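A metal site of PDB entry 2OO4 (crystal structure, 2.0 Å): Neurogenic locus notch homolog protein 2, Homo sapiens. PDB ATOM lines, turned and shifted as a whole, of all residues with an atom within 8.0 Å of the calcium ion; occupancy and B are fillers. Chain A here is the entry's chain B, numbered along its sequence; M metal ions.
A ring nitrogen (ND1) of His 91 lies within hydrogen-bond range of the backbone carbonyl oxygen (O) of Tyr 87, 2.8 Å away. The backbone carbonyl oxygen (O) of Asp 109 is in hydrogen-bond range of the backbone NH (N) of Lys 93 (3.4 Å). The backbone carbonyl oxygen of Cys 101 lies within hydrogen-bond range of the backbone NH of Asp 109 (3.2 Å). The backbone NH of Asn 98 lies within hydrogen-bond range of the side-chain sulfur of Cys 113, at 3.7 Å. The side-chain carboxylate (OD2) of Asp 112 lies close to the backbone NH (N) of Lys 93 (3.0 Å). The backbone NH (N) of Asn 95 is in hydrogen-bond range of the side-chain carboxylate (OD1) of Asp 112 (3.0 Å). The side-chain sulfur (SG) of Cys 97 is disulfide-bonded to the side-chain sulfur (SG) of Cys 113 (2.0 Å). The side-chain sulfur (SG) of Cys 88 is disulfide-bonded to the side-chain sulfur (SG) of Cys 101, 2.0 Å away.
Of the 21 residues printed, 6 come within 4 Å of the calcium ion.
The calcium ion is bound by the backbone carbonyl oxygen of His 91 (2.3 Å), the side-chain carboxylate of Asp 94 (2.3 Å), the backbone carbonyl oxygen of His 96 (2.3 Å), the side-chain carboxylate of Asp 109 (2.3 Å), the side-chain amide nitrogen of Asn 98 (2.4 Å) and the side-chain carboxylate of Asp 112 (2.5 Å). Slightly farther from the calcium ion lies the side-chain carboxylate (OD1) of Asp 109 (3.0 Å).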
ATOM      1  N   TYR A  87      23.801 -10.461 -20.103  1.00  0.00           N
ATOM      2  CA  TYR A  87      23.285 -11.010 -18.848  1.00  0.00           C
ATOM      3  C   TYR A  87      23.716 -12.458 -18.641  1.00  0.00           C
ATOM      4  O   TYR A  87      24.271 -12.803 -17.595  1.00  0.00           O
ATOM      5  CB  TYR A  87      21.761 -10.881 -18.792  1.00  0.00           C
ATOM      6  CG  TYR A  87      21.157 -11.407 -17.510  1.00  0.00           C
ATOM      7  CD1 TYR A  87      21.121 -10.618 -16.352  1.00  0.00           C
ATOM      8  CD2 TYR A  87      20.631 -12.700 -17.436  1.00  0.00           C
ATOM      9  CE1 TYR A  87      20.571 -11.098 -15.164  1.00  0.00           C
ATOM     10  CE2 TYR A  87      20.076 -13.188 -16.251  1.00  0.00           C
ATOM     11  CZ  TYR A  87      20.054 -12.394 -15.122  1.00  0.00           C
ATOM     12  OH  TYR A  87      19.515 -12.872 -13.953  1.00  0.00           O
ATOM     13  N   CYS A  88      23.472 -13.302 -19.632  1.00  0.00           N
ATOM     14  CA  CYS A  88      23.744 -14.726 -19.514  1.00  0.00           C
ATOM     15  C   CYS A  88      25.234 -15.068 -19.359  1.00  0.00           C
ATOM     16  O   CYS A  88      25.577 -15.972 -18.585  1.00  0.00           O
ATOM     17  CB  CYS A  88      23.102 -15.502 -20.665  1.00  0.00           C
ATOM     18  SG  CYS A  88      21.285 -15.539 -20.535  1.00  0.00           S
ATOM     19  N   ALA A  89      26.109 -14.333 -20.032  1.00  0.00           N
ATOM     20  CA  ALA A  89      27.554 -14.543 -19.882  1.00  0.00           C
ATOM     21  C   ALA A  89      28.012 -14.239 -18.458  1.00  0.00           C
ATOM     22  O   ALA A  89      28.864 -14.938 -17.917  1.00  0.00           O
ATOM     23  CB  ALA A  89      28.329 -13.719 -20.879  1.00  0.00           C
ATOM     24  N   ASP A  90      27.437 -13.195 -17.853  1.00  0.00           N
ATOM     25  CA  ASP A  90      27.753 -12.811 -16.475  1.00  0.00           C
ATOM     26  C   ASP A  90      27.230 -13.806 -15.437  1.00  0.00           C
ATOM     27  O   ASP A  90      27.765 -13.882 -14.324  1.00  0.00           O
ATOM     28  CB  ASP A  90      27.241 -11.403 -16.164  1.00  0.00           C
ATOM     29  CG  ASP A  90      28.113 -10.322 -16.773  1.00  0.00           C
ATOM     30  OD1 ASP A  90      29.147 -10.654 -17.382  1.00  0.00           O
ATOM     31  OD2 ASP A  90      27.779  -9.126 -16.637  1.00  0.00           O
ATOM     32  N   HIS A  91      26.198 -14.564 -15.795  1.00  0.00           N
ATOM     33  CA  HIS A  91      25.582 -15.512 -14.871  1.00  0.00           C
ATOM     34  C   HIS A  91      25.830 -16.976 -15.238  1.00  0.00           C
ATOM     35  O   HIS A  91      25.283 -17.879 -14.598  1.00  0.00           O
ATOM     36  CB  HIS A  91      24.096 -15.224 -14.724  1.00  0.00           C
ATOM     37  CG  HIS A  91      23.821 -13.874 -14.133  1.00  0.00           C
ATOM     38  ND1 HIS A  91      23.965 -12.698 -14.843  1.00  0.00           N
ATOM     39  CD2 HIS A  91      23.427 -13.514 -12.883  1.00  0.00           C
ATOM     40  CE1 HIS A  91      23.664 -11.678 -14.059  1.00  0.00           C
ATOM     41  NE2 HIS A  91      23.336 -12.139 -12.876  1.00  0.00           N
ATOM     42  N   PHE A  92      26.687 -17.189 -16.235  1.00  0.00           N
ATOM     43  CA  PHE A  92      27.130 -18.504 -16.684  1.00  0.00           C
ATOM     44  C   PHE A  92      27.938 -19.195 -15.582  1.00  0.00           C
ATOM     45  O   PHE A  92      28.895 -18.617 -15.072  1.00  0.00           O
ATOM     46  CB  PHE A  92      28.010 -18.323 -17.939  1.00  0.00           C
ATOM     47  CG  PHE A  92      28.460 -19.610 -18.580  1.00  0.00           C
ATOM     48  CD1 PHE A  92      27.667 -20.258 -19.506  1.00  0.00           C
ATOM     49  CD2 PHE A  92      29.708 -20.155 -18.272  1.00  0.00           C
ATOM     50  CE1 PHE A  92      28.086 -21.431 -20.124  1.00  0.00           C
ATOM     51  CE2 PHE A  92      30.138 -21.331 -18.868  1.00  0.00           C
ATOM     52  CZ  PHE A  92      29.336 -21.974 -19.794  1.00  0.00           C
ATOM     53  N   LYS A  93      27.540 -20.409 -15.219  1.00  0.00           N
ATOM     54  CA  LYS A  93      28.260 -21.222 -14.234  1.00  0.00           C
ATOM     55  C   LYS A  93      28.509 -20.502 -12.890  1.00  0.00           C
ATOM     56  O   LYS A  93      29.628 -20.470 -12.394  1.00  0.00           O
ATOM     57  CB  LYS A  93      29.590 -21.722 -14.837  1.00  0.00           C
ATOM     58  CG  LYS A  93      30.029 -23.104 -14.362  1.00  0.00           C
ATOM     59  CD  LYS A  93      31.307 -23.546 -15.070  1.00  0.00           C
ATOM     60  CE  LYS A  93      31.022 -24.180 -16.432  1.00  0.00           C
ATOM     61  NZ  LYS A  93      30.314 -25.502 -16.351  1.00  0.00           N
ATOM     62  N   ASP A  94      27.444 -19.941 -12.304  1.00  0.00           N
ATOM     63  CA  ASP A  94      27.591 -19.219 -11.037  1.00  0.00           C
ATOM     64  C   ASP A  94      26.885 -19.876  -9.835  1.00  0.00           C
ATOM     65  O   ASP A  94      26.608 -19.223  -8.831  1.00  0.00           O
ATOM     66  CB  ASP A  94      27.164 -17.744 -11.202  1.00  0.00           C
ATOM     67  CG  ASP A  94      25.669 -17.563 -11.423  1.00  0.00           C
ATOM     68  OD1 ASP A  94      24.952 -18.573 -11.620  1.00  0.00           O
ATOM     69  OD2 ASP A  94      25.198 -16.409 -11.394  1.00  0.00           O
ATOM     70  N   ASN A  95      26.606 -21.177  -9.964  1.00  0.00           N
ATOM     71  CA  ASN A  95      25.935 -21.977  -8.923  1.00  0.00           C
ATOM     72  C   ASN A  95      24.453 -21.641  -8.694  1.00  0.00           C
ATOM     73  O   ASN A  95      23.847 -22.085  -7.726  1.00  0.00           O
ATOM     74  CB  ASN A  95      26.710 -21.969  -7.587  1.00  0.00           C
ATOM     75  CG  ASN A  95      28.131 -22.497  -7.740  1.00  0.00           C
ATOM     76  OD1 ASN A  95      28.415 -23.322  -8.599  1.00  0.00           O
ATOM     77  ND2 ASN A  95      29.032 -22.008  -6.885  1.00  0.00           N
ATOM     78  N   HIS A  96      23.887 -20.861  -9.616  1.00  0.00           N
ATOM     79  CA  HIS A  96      22.451 -20.575  -9.611  1.00  0.00           C
ATOM     80  C   HIS A  96      21.871 -20.748 -10.997  1.00  0.00           C
ATOM     81  O   HIS A  96      22.449 -20.293 -11.987  1.00  0.00           O
ATOM     82  CB  HIS A  96      22.190 -19.148  -9.110  1.00  0.00           C
ATOM     83  CG  HIS A  96      20.756 -18.741  -9.202  1.00  0.00           C
ATOM     84  ND1 HIS A  96      19.779 -19.244  -8.379  1.00  0.00           N
ATOM     85  CD2 HIS A  96      20.136 -17.872 -10.037  1.00  0.00           C
ATOM     86  CE1 HIS A  96      18.609 -18.700  -8.698  1.00  0.00           C
ATOM     87  NE2 HIS A  96      18.807 -17.864  -9.696  1.00  0.00           N
ATOM     88  N   CYS A  97      20.724 -21.418 -11.074  1.00  0.00           N
ATOM     89  CA  CYS A  97      20.024 -21.615 -12.336  1.00  0.00           C
ATOM     90  C   CYS A  97      19.344 -20.332 -12.825  1.00  0.00           C
ATOM     91  O   CYS A  97      18.562 -19.708 -12.103  1.00  0.00           O
ATOM     92  CB  CYS A  97      18.991 -22.739 -12.211  1.00  0.00           C
ATOM     93  SG  CYS A  97      18.003 -23.025 -13.712  1.00  0.00           S
ATOM     94  N   ASN A  98      19.663 -19.953 -14.058  1.00  0.00           N
ATOM     95  CA  ASN A  98      18.985 -18.852 -14.747  1.00  0.00           C
ATOM     96  C   ASN A  98      18.283 -19.411 -15.972  1.00  0.00           C
ATOM     97  O   ASN A  98      18.942 -19.866 -16.919  1.00  0.00           O
ATOM     98  CB  ASN A  98      19.983 -17.759 -15.132  1.00  0.00           C
ATOM     99  CG  ASN A  98      20.729 -17.200 -13.934  1.00  0.00           C
ATOM    100  OD1 ASN A  98      20.233 -16.342 -13.210  1.00  0.00           O
ATOM    101  ND2 ASN A  98      21.941 -17.698 -13.722  1.00  0.00           N
ATOM    102  N   GLN A  99      16.955 -19.379 -15.953  1.00  0.00           N
ATOM    103  CA  GLN A  99      16.140 -20.019 -16.987  1.00  0.00           C
ATOM    104  C   GLN A  99      16.228 -19.335 -18.351  1.00  0.00           C
ATOM    105  O   GLN A  99      16.215 -20.004 -19.389  1.00  0.00           O
ATOM    106  CB  GLN A  99      14.682 -20.120 -16.509  1.00  0.00           C
ATOM    107  CG  GLN A  99      13.809 -21.089 -17.311  1.00  0.00           C
ATOM    108  CD  GLN A  99      14.318 -22.526 -17.313  1.00  0.00           C
ATOM    109  OE1 GLN A  99      15.050 -22.953 -16.409  1.00  0.00           O
ATOM    110  NE2 GLN A  99      13.909 -23.294 -18.312  1.00  0.00           N
ATOM    111  N   CYS A 101      18.690 -18.302 -19.618  1.00  0.00           N
ATOM    112  CA  CYS A 101      19.974 -18.741 -20.164  1.00  0.00           C
ATOM    113  C   CYS A 101      20.056 -20.259 -20.307  1.00  0.00           C
ATOM    114  O   CYS A 101      21.051 -20.787 -20.827  1.00  0.00           O
ATOM    115  CB  CYS A 101      21.119 -18.260 -19.278  1.00  0.00           C
ATOM    116  SG  CYS A 101      20.992 -16.542 -18.808  1.00  0.00           S
ATOM    117  N   TRP A 108      23.444 -23.452 -22.050  1.00  0.00           N
ATOM    118  CA  TRP A 108      22.726 -24.036 -20.921  1.00  0.00           C
ATOM    119  C   TRP A 108      23.171 -23.554 -19.534  1.00  0.00           C
ATOM    120  O   TRP A 108      23.241 -24.343 -18.578  1.00  0.00           O
ATOM    121  CB  TRP A 108      22.759 -25.567 -21.000  1.00  0.00           C
ATOM    122  CG  TRP A 108      22.051 -26.139 -22.187  1.00  0.00           C
ATOM    123  CD1 TRP A 108      20.704 -26.291 -22.340  1.00  0.00           C
ATOM    124  CD2 TRP A 108      22.652 -26.627 -23.388  1.00  0.00           C
ATOM    125  NE1 TRP A 108      20.425 -26.855 -23.560  1.00  0.00           N
ATOM    126  CE2 TRP A 108      21.601 -27.079 -24.230  1.00  0.00           C
ATOM    127  CE3 TRP A 108      23.978 -26.744 -23.840  1.00  0.00           C
ATOM    128  CZ2 TRP A 108      21.833 -27.627 -25.492  1.00  0.00           C
ATOM    129  CZ3 TRP A 108      24.201 -27.287 -25.101  1.00  0.00           C
ATOM    130  CH2 TRP A 108      23.137 -27.723 -25.908  1.00  0.00           C
ATOM    131  N   ASP A 109      23.482 -22.254 -19.444  1.00  0.00           N
ATOM    132  CA  ASP A 109      23.928 -21.605 -18.203  1.00  0.00           C
ATOM    133  C   ASP A 109      25.016 -22.384 -17.443  1.00  0.00           C
ATOM    134  O   ASP A 109      25.009 -22.455 -16.212  1.00  0.00           O
ATOM    135  CB  ASP A 109      22.726 -21.293 -17.273  1.00  0.00           C
ATOM    136  CG  ASP A 109      23.058 -20.281 -16.191  1.00  0.00           C
ATOM    137  OD1 ASP A 109      23.734 -19.276 -16.480  1.00  0.00           O
ATOM    138  OD2 ASP A 109      22.632 -20.468 -15.025  1.00  0.00           O
ATOM    139  N   GLY A 110      25.954 -22.964 -18.203  1.00  0.00           N
ATOM    140  CA  GLY A 110      27.076 -23.709 -17.629  1.00  0.00           C
ATOM    141  C   GLY A 110      26.683 -24.879 -16.739  1.00  0.00           C
ATOM    142  O   GLY A 110      27.400 -25.207 -15.792  1.00  0.00           O
ATOM    143  N   LEU A 111      25.537 -25.488 -17.051  1.00  0.00           N
ATOM    144  CA  LEU A 111      24.989 -26.624 -16.309  1.00  0.00           C
ATOM    145  C   LEU A 111      24.515 -26.300 -14.870  1.00  0.00           C
ATOM    146  O   LEU A 111      24.330 -27.211 -14.054  1.00  0.00           O
ATOM    147  CB  LEU A 111      25.956 -27.817 -16.314  1.00  0.00           C
ATOM    148  CG  LEU A 111      26.331 -28.453 -17.660  1.00  0.00           C
ATOM    149  CD1 LEU A 111      27.390 -29.521 -17.472  1.00  0.00           C
ATOM    150  CD2 LEU A 111      25.108 -29.010 -18.381  1.00  0.00           C
ATOM    151  N   ASP A 112      24.311 -25.011 -14.599  1.00  0.00           N
ATOM    152  CA  ASP A 112      23.801 -24.551 -13.299  1.00  0.00           C
ATOM    153  C   ASP A 112      22.403 -25.077 -13.000  1.00  0.00           C
ATOM    154  O   ASP A 112      21.972 -25.117 -11.838  1.00  0.00           O
ATOM    155  CB  ASP A 112      23.744 -23.022 -13.245  1.00  0.00           C
ATOM    156  CG  ASP A 112      25.097 -22.378 -12.956  1.00  0.00           C
ATOM    157  OD1 ASP A 112      25.944 -22.987 -12.279  1.00  0.00           O
ATOM    158  OD2 ASP A 112      25.283 -21.224 -13.401  1.00  0.00           O
ATOM    159  N   CYS A 113      21.680 -25.444 -14.056  1.00  0.00           N
ATOM    160  CA  CYS A 113      20.305 -25.934 -13.934  1.00  0.00           C
ATOM    161  C   CYS A 113      20.237 -27.469 -13.964  1.00  0.00           C
ATOM    162  O   CYS A 113      19.194 -28.047 -13.665  1.00  0.00           O
ATOM    163  CB  CYS A 113      19.424 -25.344 -15.048  1.00  0.00           C
ATOM    164  SG  CYS A 113      19.393 -23.512 -15.091  1.00  0.00           S
ATOM    165  N   ARG A 142      35.285 -19.364 -16.804  1.00  0.00           N
ATOM    166  CA  ARG A 142      33.859 -19.370 -17.153  1.00  0.00           C
ATOM    167  C   ARG A 142      33.610 -18.862 -18.570  1.00  0.00           C
ATOM    168  O   ARG A 142      32.943 -19.534 -19.360  1.00  0.00           O
ATOM    169  CB  ARG A 142      33.052 -18.523 -16.157  1.00  0.00           C
ATOM    170  CG  ARG A 142      32.820 -19.182 -14.816  1.00  0.00           C
ATOM    171  CD  ARG A 142      32.523 -18.128 -13.743  1.00  0.00           C
ATOM    172  NE  ARG A 142      31.128 -17.697 -13.736  1.00  0.00           N
ATOM    173  CZ  ARG A 142      30.691 -16.512 -14.172  1.00  0.00           C
ATOM    174  NH1 ARG A 142      31.534 -15.607 -14.664  1.00  0.00           N
ATOM    175  NH2 ARG A 142      29.397 -16.237 -14.119  1.00  0.00           N
HETATM  176 CA    CA M   1      23.846 -19.203 -13.479  1.00  0.00          CA
